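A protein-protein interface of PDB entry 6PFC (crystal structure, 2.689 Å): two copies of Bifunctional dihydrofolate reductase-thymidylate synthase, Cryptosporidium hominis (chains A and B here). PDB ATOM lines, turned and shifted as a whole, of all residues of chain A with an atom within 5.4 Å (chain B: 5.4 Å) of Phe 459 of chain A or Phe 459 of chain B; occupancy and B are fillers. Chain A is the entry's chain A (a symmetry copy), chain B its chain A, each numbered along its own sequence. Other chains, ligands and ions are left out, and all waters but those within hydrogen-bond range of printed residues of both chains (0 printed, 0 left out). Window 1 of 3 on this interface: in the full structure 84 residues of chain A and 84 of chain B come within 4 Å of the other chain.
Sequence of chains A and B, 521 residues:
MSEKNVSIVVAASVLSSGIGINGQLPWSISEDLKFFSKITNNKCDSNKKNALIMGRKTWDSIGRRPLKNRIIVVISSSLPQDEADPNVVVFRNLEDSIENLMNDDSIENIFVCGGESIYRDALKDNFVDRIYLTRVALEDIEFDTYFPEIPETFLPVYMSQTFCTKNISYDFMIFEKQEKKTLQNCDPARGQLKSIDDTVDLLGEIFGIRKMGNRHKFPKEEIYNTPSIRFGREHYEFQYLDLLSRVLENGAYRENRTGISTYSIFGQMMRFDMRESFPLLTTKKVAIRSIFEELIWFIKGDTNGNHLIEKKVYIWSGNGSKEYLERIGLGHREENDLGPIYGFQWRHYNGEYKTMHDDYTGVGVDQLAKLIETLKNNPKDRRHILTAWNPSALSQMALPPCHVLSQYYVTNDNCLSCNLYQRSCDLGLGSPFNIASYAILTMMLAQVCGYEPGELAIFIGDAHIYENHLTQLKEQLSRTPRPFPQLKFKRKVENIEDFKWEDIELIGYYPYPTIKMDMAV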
ATOM      1  N   GLY A 267       5.637  19.032 -31.592  1.00  0.00           N
ATOM      2  CA  GLY A 267       5.005  19.760 -30.508  1.00  0.00           C
ATOM      3  C   GLY A 267       5.954  20.436 -29.538  1.00  0.00           C
ATOM      4  O   GLY A 267       6.253  19.893 -28.470  1.00  0.00           O
ATOM      5  N   GLN A 268       6.427  21.630 -29.889  1.00  0.00           N
ATOM      6  CA  GLN A 268       7.324  22.390 -29.031  1.00  0.00           C
ATOM      7  C   GLN A 268       6.894  23.852 -29.032  1.00  0.00           C
ATOM      8  O   GLN A 268       6.026  24.266 -29.804  1.00  0.00           O
ATOM      9  CB  GLN A 268       8.783  22.245 -29.479  1.00  0.00           C
ATOM     10  CG  GLN A 268       9.332  20.831 -29.333  1.00  0.00           C
ATOM     11  CD  GLN A 268       9.541  20.437 -27.885  1.00  0.00           C
ATOM     12  OE1 GLN A 268      10.056  21.219 -27.088  1.00  0.00           O
ATOM     13  NE2 GLN A 268       9.138  19.221 -27.536  1.00  0.00           N
ATOM     14  N   MET A 269       7.507  24.636 -28.146  1.00  0.00           N
ATOM     15  CA  MET A 269       7.192  26.055 -28.058  1.00  0.00           C
ATOM     16  C   MET A 269       8.394  26.817 -27.519  1.00  0.00           C
ATOM     17  O   MET A 269       9.261  26.258 -26.842  1.00  0.00           O
ATOM     18  CB  MET A 269       5.969  26.323 -27.172  1.00  0.00           C
ATOM     19  CG  MET A 269       6.274  26.372 -25.685  1.00  0.00           C
ATOM     20  SD  MET A 269       4.963  27.189 -24.754  1.00  0.00           S
ATOM     21  CE  MET A 269       5.597  27.061 -23.085  1.00  0.00           C
ATOM     22  N   MET A 270       8.423  28.114 -27.823  1.00  0.00           N
ATOM     23  CA  MET A 270       9.474  29.015 -27.372  1.00  0.00           C
ATOM     24  C   MET A 270       8.856  30.352 -26.994  1.00  0.00           C
ATOM     25  O   MET A 270       7.970  30.851 -27.694  1.00  0.00           O
ATOM     26  CB  MET A 270      10.538  29.230 -28.456  1.00  0.00           C
ATOM     27  CG  MET A 270      11.296  27.984 -28.867  1.00  0.00           C
ATOM     28  SD  MET A 270      12.489  28.320 -30.180  1.00  0.00           S
ATOM     29  CE  MET A 270      11.394  28.798 -31.515  1.00  0.00           C
ATOM     30  N   ASN A 419       1.421  35.434 -30.914  1.00  0.00           N
ATOM     31  CA  ASN A 419       1.557  33.986 -30.988  1.00  0.00           C
ATOM     32  C   ASN A 419       1.669  33.571 -32.448  1.00  0.00           C
ATOM     33  O   ASN A 419       0.972  34.112 -33.310  1.00  0.00           O
ATOM     34  CB  ASN A 419       0.367  33.266 -30.346  1.00  0.00           C
ATOM     35  CG  ASN A 419       0.436  33.254 -28.838  1.00  0.00           C
ATOM     36  OD1 ASN A 419       1.473  33.557 -28.251  1.00  0.00           O
ATOM     37  ND2 ASN A 419      -0.669  32.890 -28.200  1.00  0.00           N
ATOM     38  N   LEU A 420       2.544  32.607 -32.720  1.00  0.00           N
ATOM     39  CA  LEU A 420       2.757  32.105 -34.070  1.00  0.00           C
ATOM     40  C   LEU A 420       2.790  30.585 -34.042  1.00  0.00           C
ATOM     41  O   LEU A 420       3.523  29.994 -33.244  1.00  0.00           O
ATOM     42  CB  LEU A 420       4.062  32.644 -34.661  1.00  0.00           C
ATOM     43  CG  LEU A 420       4.534  31.926 -35.926  1.00  0.00           C
ATOM     44  CD1 LEU A 420       3.581  32.191 -37.082  1.00  0.00           C
ATOM     45  CD2 LEU A 420       5.956  32.334 -36.280  1.00  0.00           C
ATOM     46  N   TYR A 421       2.008  29.957 -34.917  1.00  0.00           N
ATOM     47  CA  TYR A 421       2.071  28.516 -35.114  1.00  0.00           C
ATOM     48  C   TYR A 421       2.827  28.210 -36.398  1.00  0.00           C
ATOM     49  O   TYR A 421       2.513  28.762 -37.459  1.00  0.00           O
ATOM     50  CB  TYR A 421       0.677  27.885 -35.163  1.00  0.00           C
ATOM     51  CG  TYR A 421       0.736  26.376 -35.225  1.00  0.00           C
ATOM     52  CD1 TYR A 421       0.900  25.623 -34.069  1.00  0.00           C
ATOM     53  CD2 TYR A 421       0.654  25.704 -36.438  1.00  0.00           C
ATOM     54  CE1 TYR A 421       0.969  24.242 -34.119  1.00  0.00           C
ATOM     55  CE2 TYR A 421       0.721  24.323 -36.497  1.00  0.00           C
ATOM     56  CZ  TYR A 421       0.879  23.598 -35.334  1.00  0.00           C
ATOM     57  OH  TYR A 421       0.947  22.225 -35.386  1.00  0.00           O
ATOM     58  N   GLN A 422       3.820  27.329 -36.299  1.00  0.00           N
ATOM     59  CA  GLN A 422       4.680  26.962 -37.417  1.00  0.00           C
ATOM     60  C   GLN A 422       4.588  25.458 -37.631  1.00  0.00           C
ATOM     61  O   GLN A 422       4.925  24.679 -36.733  1.00  0.00           O
ATOM     62  CB  GLN A 422       6.125  27.388 -37.149  1.00  0.00           C
ATOM     63  CG  GLN A 422       7.069  27.182 -38.316  1.00  0.00           C
ATOM     64  CD  GLN A 422       8.452  27.739 -38.044  1.00  0.00           C
ATOM     65  OE1 GLN A 422       8.777  28.096 -36.912  1.00  0.00           O
ATOM     66  NE2 GLN A 422       9.274  27.817 -39.082  1.00  0.00           N
ATOM     67  N   ALA A 457       5.539  34.284 -28.574  1.00  0.00           N
ATOM     68  CA  ALA A 457       5.487  32.844 -28.368  1.00  0.00           C
ATOM     69  C   ALA A 457       5.318  32.153 -29.714  1.00  0.00           C
ATOM     70  O   ALA A 457       4.433  32.515 -30.496  1.00  0.00           O
ATOM     71  CB  ALA A 457       4.347  32.463 -27.423  1.00  0.00           C
ATOM     72  N   ILE A 458       6.162  31.160 -29.978  1.00  0.00           N
ATOM     73  CA  ILE A 458       6.145  30.422 -31.234  1.00  0.00           C
ATOM     74  C   ILE A 458       5.852  28.963 -30.918  1.00  0.00           C
ATOM     75  O   ILE A 458       6.621  28.312 -30.200  1.00  0.00           O
ATOM     76  CB  ILE A 458       7.471  30.559 -31.998  1.00  0.00           C
ATOM     77  CG1 ILE A 458       7.734  32.024 -32.353  1.00  0.00           C
ATOM     78  CG2 ILE A 458       7.454  29.698 -33.252  1.00  0.00           C
ATOM     79  CD1 ILE A 458       9.055  32.253 -33.057  1.00  0.00           C
ATOM     80  N   PHE A 459       4.745  28.453 -31.450  1.00  0.00           N
ATOM     81  CA  PHE A 459       4.354  27.062 -31.266  1.00  0.00           C
ATOM     82  C   PHE A 459       4.672  26.284 -32.538  1.00  0.00           C
ATOM     83  O   PHE A 459       4.224  26.654 -33.628  1.00  0.00           O
ATOM     84  CB  PHE A 459       2.869  26.949 -30.923  1.00  0.00           C
ATOM     85  CG  PHE A 459       2.445  27.824 -29.777  1.00  0.00           C
ATOM     86  CD1 PHE A 459       2.906  27.579 -28.494  1.00  0.00           C
ATOM     87  CD2 PHE A 459       1.574  28.882 -29.979  1.00  0.00           C
ATOM     88  CE1 PHE A 459       2.515  28.377 -27.435  1.00  0.00           C
ATOM     89  CE2 PHE A 459       1.178  29.684 -28.923  1.00  0.00           C
ATOM     90  CZ  PHE A 459       1.649  29.431 -27.650  1.00  0.00           C
ATOM     91  N   ILE A 460       5.431  25.202 -32.392  1.00  0.00           N
ATOM     92  CA  ILE A 460       6.033  24.502 -33.520  1.00  0.00           C
ATOM     93  C   ILE A 460       5.427  23.112 -33.641  1.00  0.00           C
ATOM     94  O   ILE A 460       5.258  22.403 -32.641  1.00  0.00           O
ATOM     95  CB  ILE A 460       7.564  24.421 -33.363  1.00  0.00           C
ATOM     96  CG1 ILE A 460       8.168  25.827 -33.325  1.00  0.00           C
ATOM     97  CG2 ILE A 460       8.176  23.592 -34.480  1.00  0.00           C
ATOM     98  CD1 ILE A 460       9.665  25.845 -33.111  1.00  0.00           C
ATOM     99  N   GLY A 461       5.105  22.724 -34.873  1.00  0.00           N
ATOM    100  CA  GLY A 461       4.688  21.368 -35.165  1.00  0.00           C
ATOM    101  C   GLY A 461       5.871  20.440 -35.348  1.00  0.00           C
ATOM    102  O   GLY A 461       6.347  19.839 -34.380  1.00  0.00           O
ATOM    103  N   GLY B 267      -0.908  32.982 -24.482  1.00  0.00           N
ATOM    104  CA  GLY B 267       0.184  32.085 -24.811  1.00  0.00           C
ATOM    105  C   GLY B 267       0.431  30.970 -23.816  1.00  0.00           C
ATOM    106  O   GLY B 267       1.308  31.079 -22.953  1.00  0.00           O
ATOM    107  N   GLN B 268      -0.325  29.879 -23.930  1.00  0.00           N
ATOM    108  CA  GLN B 268      -0.165  28.730 -23.051  1.00  0.00           C
ATOM    109  C   GLN B 268      -0.241  27.455 -23.881  1.00  0.00           C
ATOM    110  O   GLN B 268      -0.567  27.479 -25.070  1.00  0.00           O
ATOM    111  CB  GLN B 268      -1.219  28.726 -21.937  1.00  0.00           C
ATOM    112  CG  GLN B 268      -1.085  29.888 -20.962  1.00  0.00           C
ATOM    113  CD  GLN B 268       0.132  29.758 -20.068  1.00  0.00           C
ATOM    114  OE1 GLN B 268       0.419  28.681 -19.548  1.00  0.00           O
ATOM    115  NE2 GLN B 268       0.857  30.855 -19.887  1.00  0.00           N
ATOM    116  N   MET B 269       0.075  26.328 -23.242  1.00  0.00           N
ATOM    117  CA  MET B 269       0.028  25.042 -23.923  1.00  0.00           C
ATOM    118  C   MET B 269      -0.231  23.934 -22.914  1.00  0.00           C
ATOM    119  O   MET B 269       0.042  24.073 -21.719  1.00  0.00           O
ATOM    120  CB  MET B 269       1.321  24.749 -24.694  1.00  0.00           C
ATOM    121  CG  MET B 269       2.440  24.176 -23.842  1.00  0.00           C
ATOM    122  SD  MET B 269       3.708  23.375 -24.845  1.00  0.00           S
ATOM    123  CE  MET B 269       4.860  22.846 -23.580  1.00  0.00           C
ATOM    124  N   MET B 270      -0.754  22.819 -23.422  1.00  0.00           N
ATOM    125  CA  MET B 270      -1.043  21.637 -22.622  1.00  0.00           C
ATOM    126  C   MET B 270      -0.680  20.394 -23.419  1.00  0.00           C
ATOM    127  O   MET B 270      -0.952  20.321 -24.620  1.00  0.00           O
ATOM    128  CB  MET B 270      -2.522  21.575 -22.219  1.00  0.00           C
ATOM    129  CG  MET B 270      -2.998  22.717 -21.344  1.00  0.00           C
ATOM    130  SD  MET B 270      -4.758  22.590 -20.963  1.00  0.00           S
ATOM    131  CE  MET B 270      -5.470  22.776 -22.596  1.00  0.00           C
ATOM    132  N   ASN B 419      -1.459  18.335 -32.991  1.00  0.00           N
ATOM    133  CA  ASN B 419      -1.311  19.678 -32.448  1.00  0.00           C
ATOM    134  C   ASN B 419      -2.535  20.503 -32.816  1.00  0.00           C
ATOM    135  O   ASN B 419      -3.045  20.405 -33.935  1.00  0.00           O
ATOM    136  CB  ASN B 419      -0.053  20.373 -32.979  1.00  0.00           C
ATOM    137  CG  ASN B 419       1.208  19.895 -32.301  1.00  0.00           C
ATOM    138  OD1 ASN B 419       1.158  19.230 -31.269  1.00  0.00           O
ATOM    139  ND2 ASN B 419       2.354  20.244 -32.874  1.00  0.00           N
ATOM    140  N   LEU B 420      -3.002  21.316 -31.874  1.00  0.00           N
ATOM    141  CA  LEU B 420      -4.164  22.168 -32.083  1.00  0.00           C
ATOM    142  C   LEU B 420      -3.864  23.565 -31.564  1.00  0.00           C
ATOM    143  O   LEU B 420      -3.418  23.722 -30.424  1.00  0.00           O
ATOM    144  CB  LEU B 420      -5.399  21.602 -31.376  1.00  0.00           C
ATOM    145  CG  LEU B 420      -6.570  22.577 -31.259  1.00  0.00           C
ATOM    146  CD1 LEU B 420      -7.156  22.879 -32.631  1.00  0.00           C
ATOM    147  CD2 LEU B 420      -7.632  22.038 -30.314  1.00  0.00           C
ATOM    148  N   TYR B 421      -4.120  24.575 -32.392  1.00  0.00           N
ATOM    149  CA  TYR B 421      -4.042  25.964 -31.964  1.00  0.00           C
ATOM    150  C   TYR B 421      -5.445  26.508 -31.743  1.00  0.00           C
ATOM    151  O   TYR B 421      -6.310  26.390 -32.619  1.00  0.00           O
ATOM    152  CB  TYR B 421      -3.296  26.833 -32.980  1.00  0.00           C
ATOM    153  CG  TYR B 421      -3.088  28.244 -32.478  1.00  0.00           C
ATOM    154  CD1 TYR B 421      -2.031  28.548 -31.629  1.00  0.00           C
ATOM    155  CD2 TYR B 421      -3.959  29.267 -32.832  1.00  0.00           C
ATOM    156  CE1 TYR B 421      -1.841  29.833 -31.155  1.00  0.00           C
ATOM    157  CE2 TYR B 421      -3.776  30.556 -32.363  1.00  0.00           C
ATOM    158  CZ  TYR B 421      -2.716  30.832 -31.525  1.00  0.00           C
ATOM    159  OH  TYR B 421      -2.529  32.111 -31.054  1.00  0.00           O
ATOM    160  N   GLN B 422      -5.666  27.104 -30.574  1.00  0.00           N
ATOM    161  CA  GLN B 422      -6.965  27.633 -30.177  1.00  0.00           C
ATOM    162  C   GLN B 422      -6.816  29.117 -29.869  1.00  0.00           C
ATOM    163  O   GLN B 422      -6.058  29.493 -28.968  1.00  0.00           O
ATOM    164  CB  GLN B 422      -7.508  26.875 -28.964  1.00  0.00           C
ATOM    165  CG  GLN B 422      -8.920  27.253 -28.565  1.00  0.00           C
ATOM    166  CD  GLN B 422      -9.455  26.384 -27.445  1.00  0.00           C
ATOM    167  OE1 GLN B 422      -8.709  25.633 -26.817  1.00  0.00           O
ATOM    168  NE2 GLN B 422     -10.754  26.482 -27.188  1.00  0.00           N
ATOM    169  N   ALA B 457      -1.203  17.875 -28.146  1.00  0.00           N
ATOM    170  CA  ALA B 457      -0.726  19.159 -27.652  1.00  0.00           C
ATOM    171  C   ALA B 457      -1.665  20.257 -28.127  1.00  0.00           C
ATOM    172  O   ALA B 457      -1.982  20.337 -29.318  1.00  0.00           O
ATOM    173  CB  ALA B 457       0.703  19.433 -28.124  1.00  0.00           C
ATOM    174  N   ILE B 458      -2.104  21.101 -27.199  1.00  0.00           N
ATOM    175  CA  ILE B 458      -3.031  22.187 -27.492  1.00  0.00           C
ATOM    176  C   ILE B 458      -2.339  23.499 -27.155  1.00  0.00           C
ATOM    177  O   ILE B 458      -1.967  23.730 -25.998  1.00  0.00           O
ATOM    178  CB  ILE B 458      -4.347  22.046 -26.710  1.00  0.00           C
ATOM    179  CG1 ILE B 458      -5.058  20.746 -27.091  1.00  0.00           C
ATOM    180  CG2 ILE B 458      -5.247  23.244 -26.965  1.00  0.00           C
ATOM    181  CD1 ILE B 458      -6.336  20.501 -26.319  1.00  0.00           C
ATOM    182  N   PHE B 459      -2.168  24.353 -28.159  1.00  0.00           N
ATOM    183  CA  PHE B 459      -1.557  25.664 -27.980  1.00  0.00           C
ATOM    184  C   PHE B 459      -2.649  26.726 -27.981  1.00  0.00           C
ATOM    185  O   PHE B 459      -3.440  26.812 -28.926  1.00  0.00           O
ATOM    186  CB  PHE B 459      -0.531  25.945 -29.078  1.00  0.00           C
ATOM    187  CG  PHE B 459       0.486  24.852 -29.250  1.00  0.00           C
ATOM    188  CD1 PHE B 459       1.412  24.586 -28.255  1.00  0.00           C
ATOM    189  CD2 PHE B 459       0.526  24.100 -30.412  1.00  0.00           C
ATOM    190  CE1 PHE B 459       2.353  23.586 -28.410  1.00  0.00           C
ATOM    191  CE2 PHE B 459       1.467  23.097 -30.574  1.00  0.00           C
ATOM    192  CZ  PHE B 459       2.381  22.841 -29.572  1.00  0.00           C
ATOM    193  N   ILE B 460      -2.680  27.541 -26.930  1.00  0.00           N
ATOM    194  CA  ILE B 460      -3.799  28.431 -26.653  1.00  0.00           C
ATOM    195  C   ILE B 460      -3.347  29.878 -26.783  1.00  0.00           C
ATOM    196  O   ILE B 460      -2.273  30.253 -26.297  1.00  0.00           O
ATOM    197  CB  ILE B 460      -4.382  28.162 -25.252  1.00  0.00           C
ATOM    198  CG1 ILE B 460      -4.908  26.728 -25.162  1.00  0.00           C
ATOM    199  CG2 ILE B 460      -5.472  29.168 -24.921  1.00  0.00           C
ATOM    200  CD1 ILE B 460      -5.444  26.356 -23.797  1.00  0.00           C
ATOM    201  N   GLY B 461      -4.174  30.688 -27.439  1.00  0.00           N
ATOM    202  CA  GLY B 461      -3.965  32.120 -27.488  1.00  0.00           C
ATOM    203  C   GLY B 461      -4.510  32.814 -26.256  1.00  0.00           C
ATOM    204  O   GLY B 461      -3.792  32.976 -25.264  1.00  0.00           O
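Among the printed residues, merely in contact across the chains: Phe 459 of chain A with Phe 459 of chain B, Gly 461 of chain A with Asn 419 of chain B, Asn 419 of chain A with Gly 461 of chain B, Gly 267 of chain A with Asn 419 of chain B, Asn 419 of chain A with Gly 267 of chain B, Asn 419 of chain A with Ile 460 of chain B, Ile 460 of chain A with Asn 419 of chain B, Phe 459 of chain A with Tyr 421 of chain B, Tyr 421 of chain A with Phe 459 of chain B, Gln 268 of chain A with Phe 459 of chain B and Phe 459 of chain A with Gln 268 of chain B.
N of Ile 460 of chain B is in hydrogen-bond range of O of Gln 268 of chain B.
O of Leu 420 of chain B sits at hydrogen-bond distance from N of Phe 459 of chain B.
The backbone carbonyl oxygen (O) of Phe 459 of chain B is in hydrogen-bond range of the backbone NH (N) of Gln 422 of chain B, at 2.8 Å.
O of Gln 422 of chain B sits at hydrogen-bond distance from N of Gly 461 of chain B, at 2.7 Å.
O of Gly 461 of chain A sits at hydrogen-bond distance from N of Gly 267 of chain A.
N of Gly 461 of chain A lies within hydrogen-bond range of O of Gln 422 of chain A (2.7 Å).
Gly 267 of chain A touches Asn 419 of chain B, and with the chains exchanged Asn 419 of chain A touches Gly 267 of chain B.
Gln 268 of chain A touches Phe 459 of chain B, and with the chains exchanged Phe 459 of chain A touches Gln 268 of chain B.
Asn 419 of chain A touches Tyr 421 of chain B, and with the chains exchanged Tyr 421 of chain A touches Asn 419 of chain B.
Phe 459 of chain A touches its own counterpart, Phe 459 of chain B.
Positions printed for both chains: 267, 268, 269, 270, 419, 420, 421, 422, 457, 458, 459, 460 and 461.
Of the 13 printed residues of chain B, 7 touch a printed residue of chain A.
Hydrophobic or aromatic side chains of chain B that line the printed part of chain A: Tyr 421 and Phe 459.
Along chain B the printed residues that touch a printed residue of chain A span positions 267 to 461.
Phe 459 of chain A touches just these residues of chain B: Gln 268 (3.9 Å), Tyr 421 (3.7 Å) and Phe 459 (3.4 Å).
Of the printed residues of chain A, Tyr 421 of chain B touches Asn 419 and Phe 459.
Gln 422 of chain B touches none of the printed residues of chain A.
Of the printed residues of chain A, Gly 461 of chain B touches Asn 419 (3.5 Å).
OH of Tyr 421 of chain A sits close to ND2 of Asn 419 of chain B (3.5 Å).
The side-chain amide nitrogen (ND2) of Asn 419 of chain A lies close to the side-chain hydroxyl (OH) of Tyr 421 of chain B.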
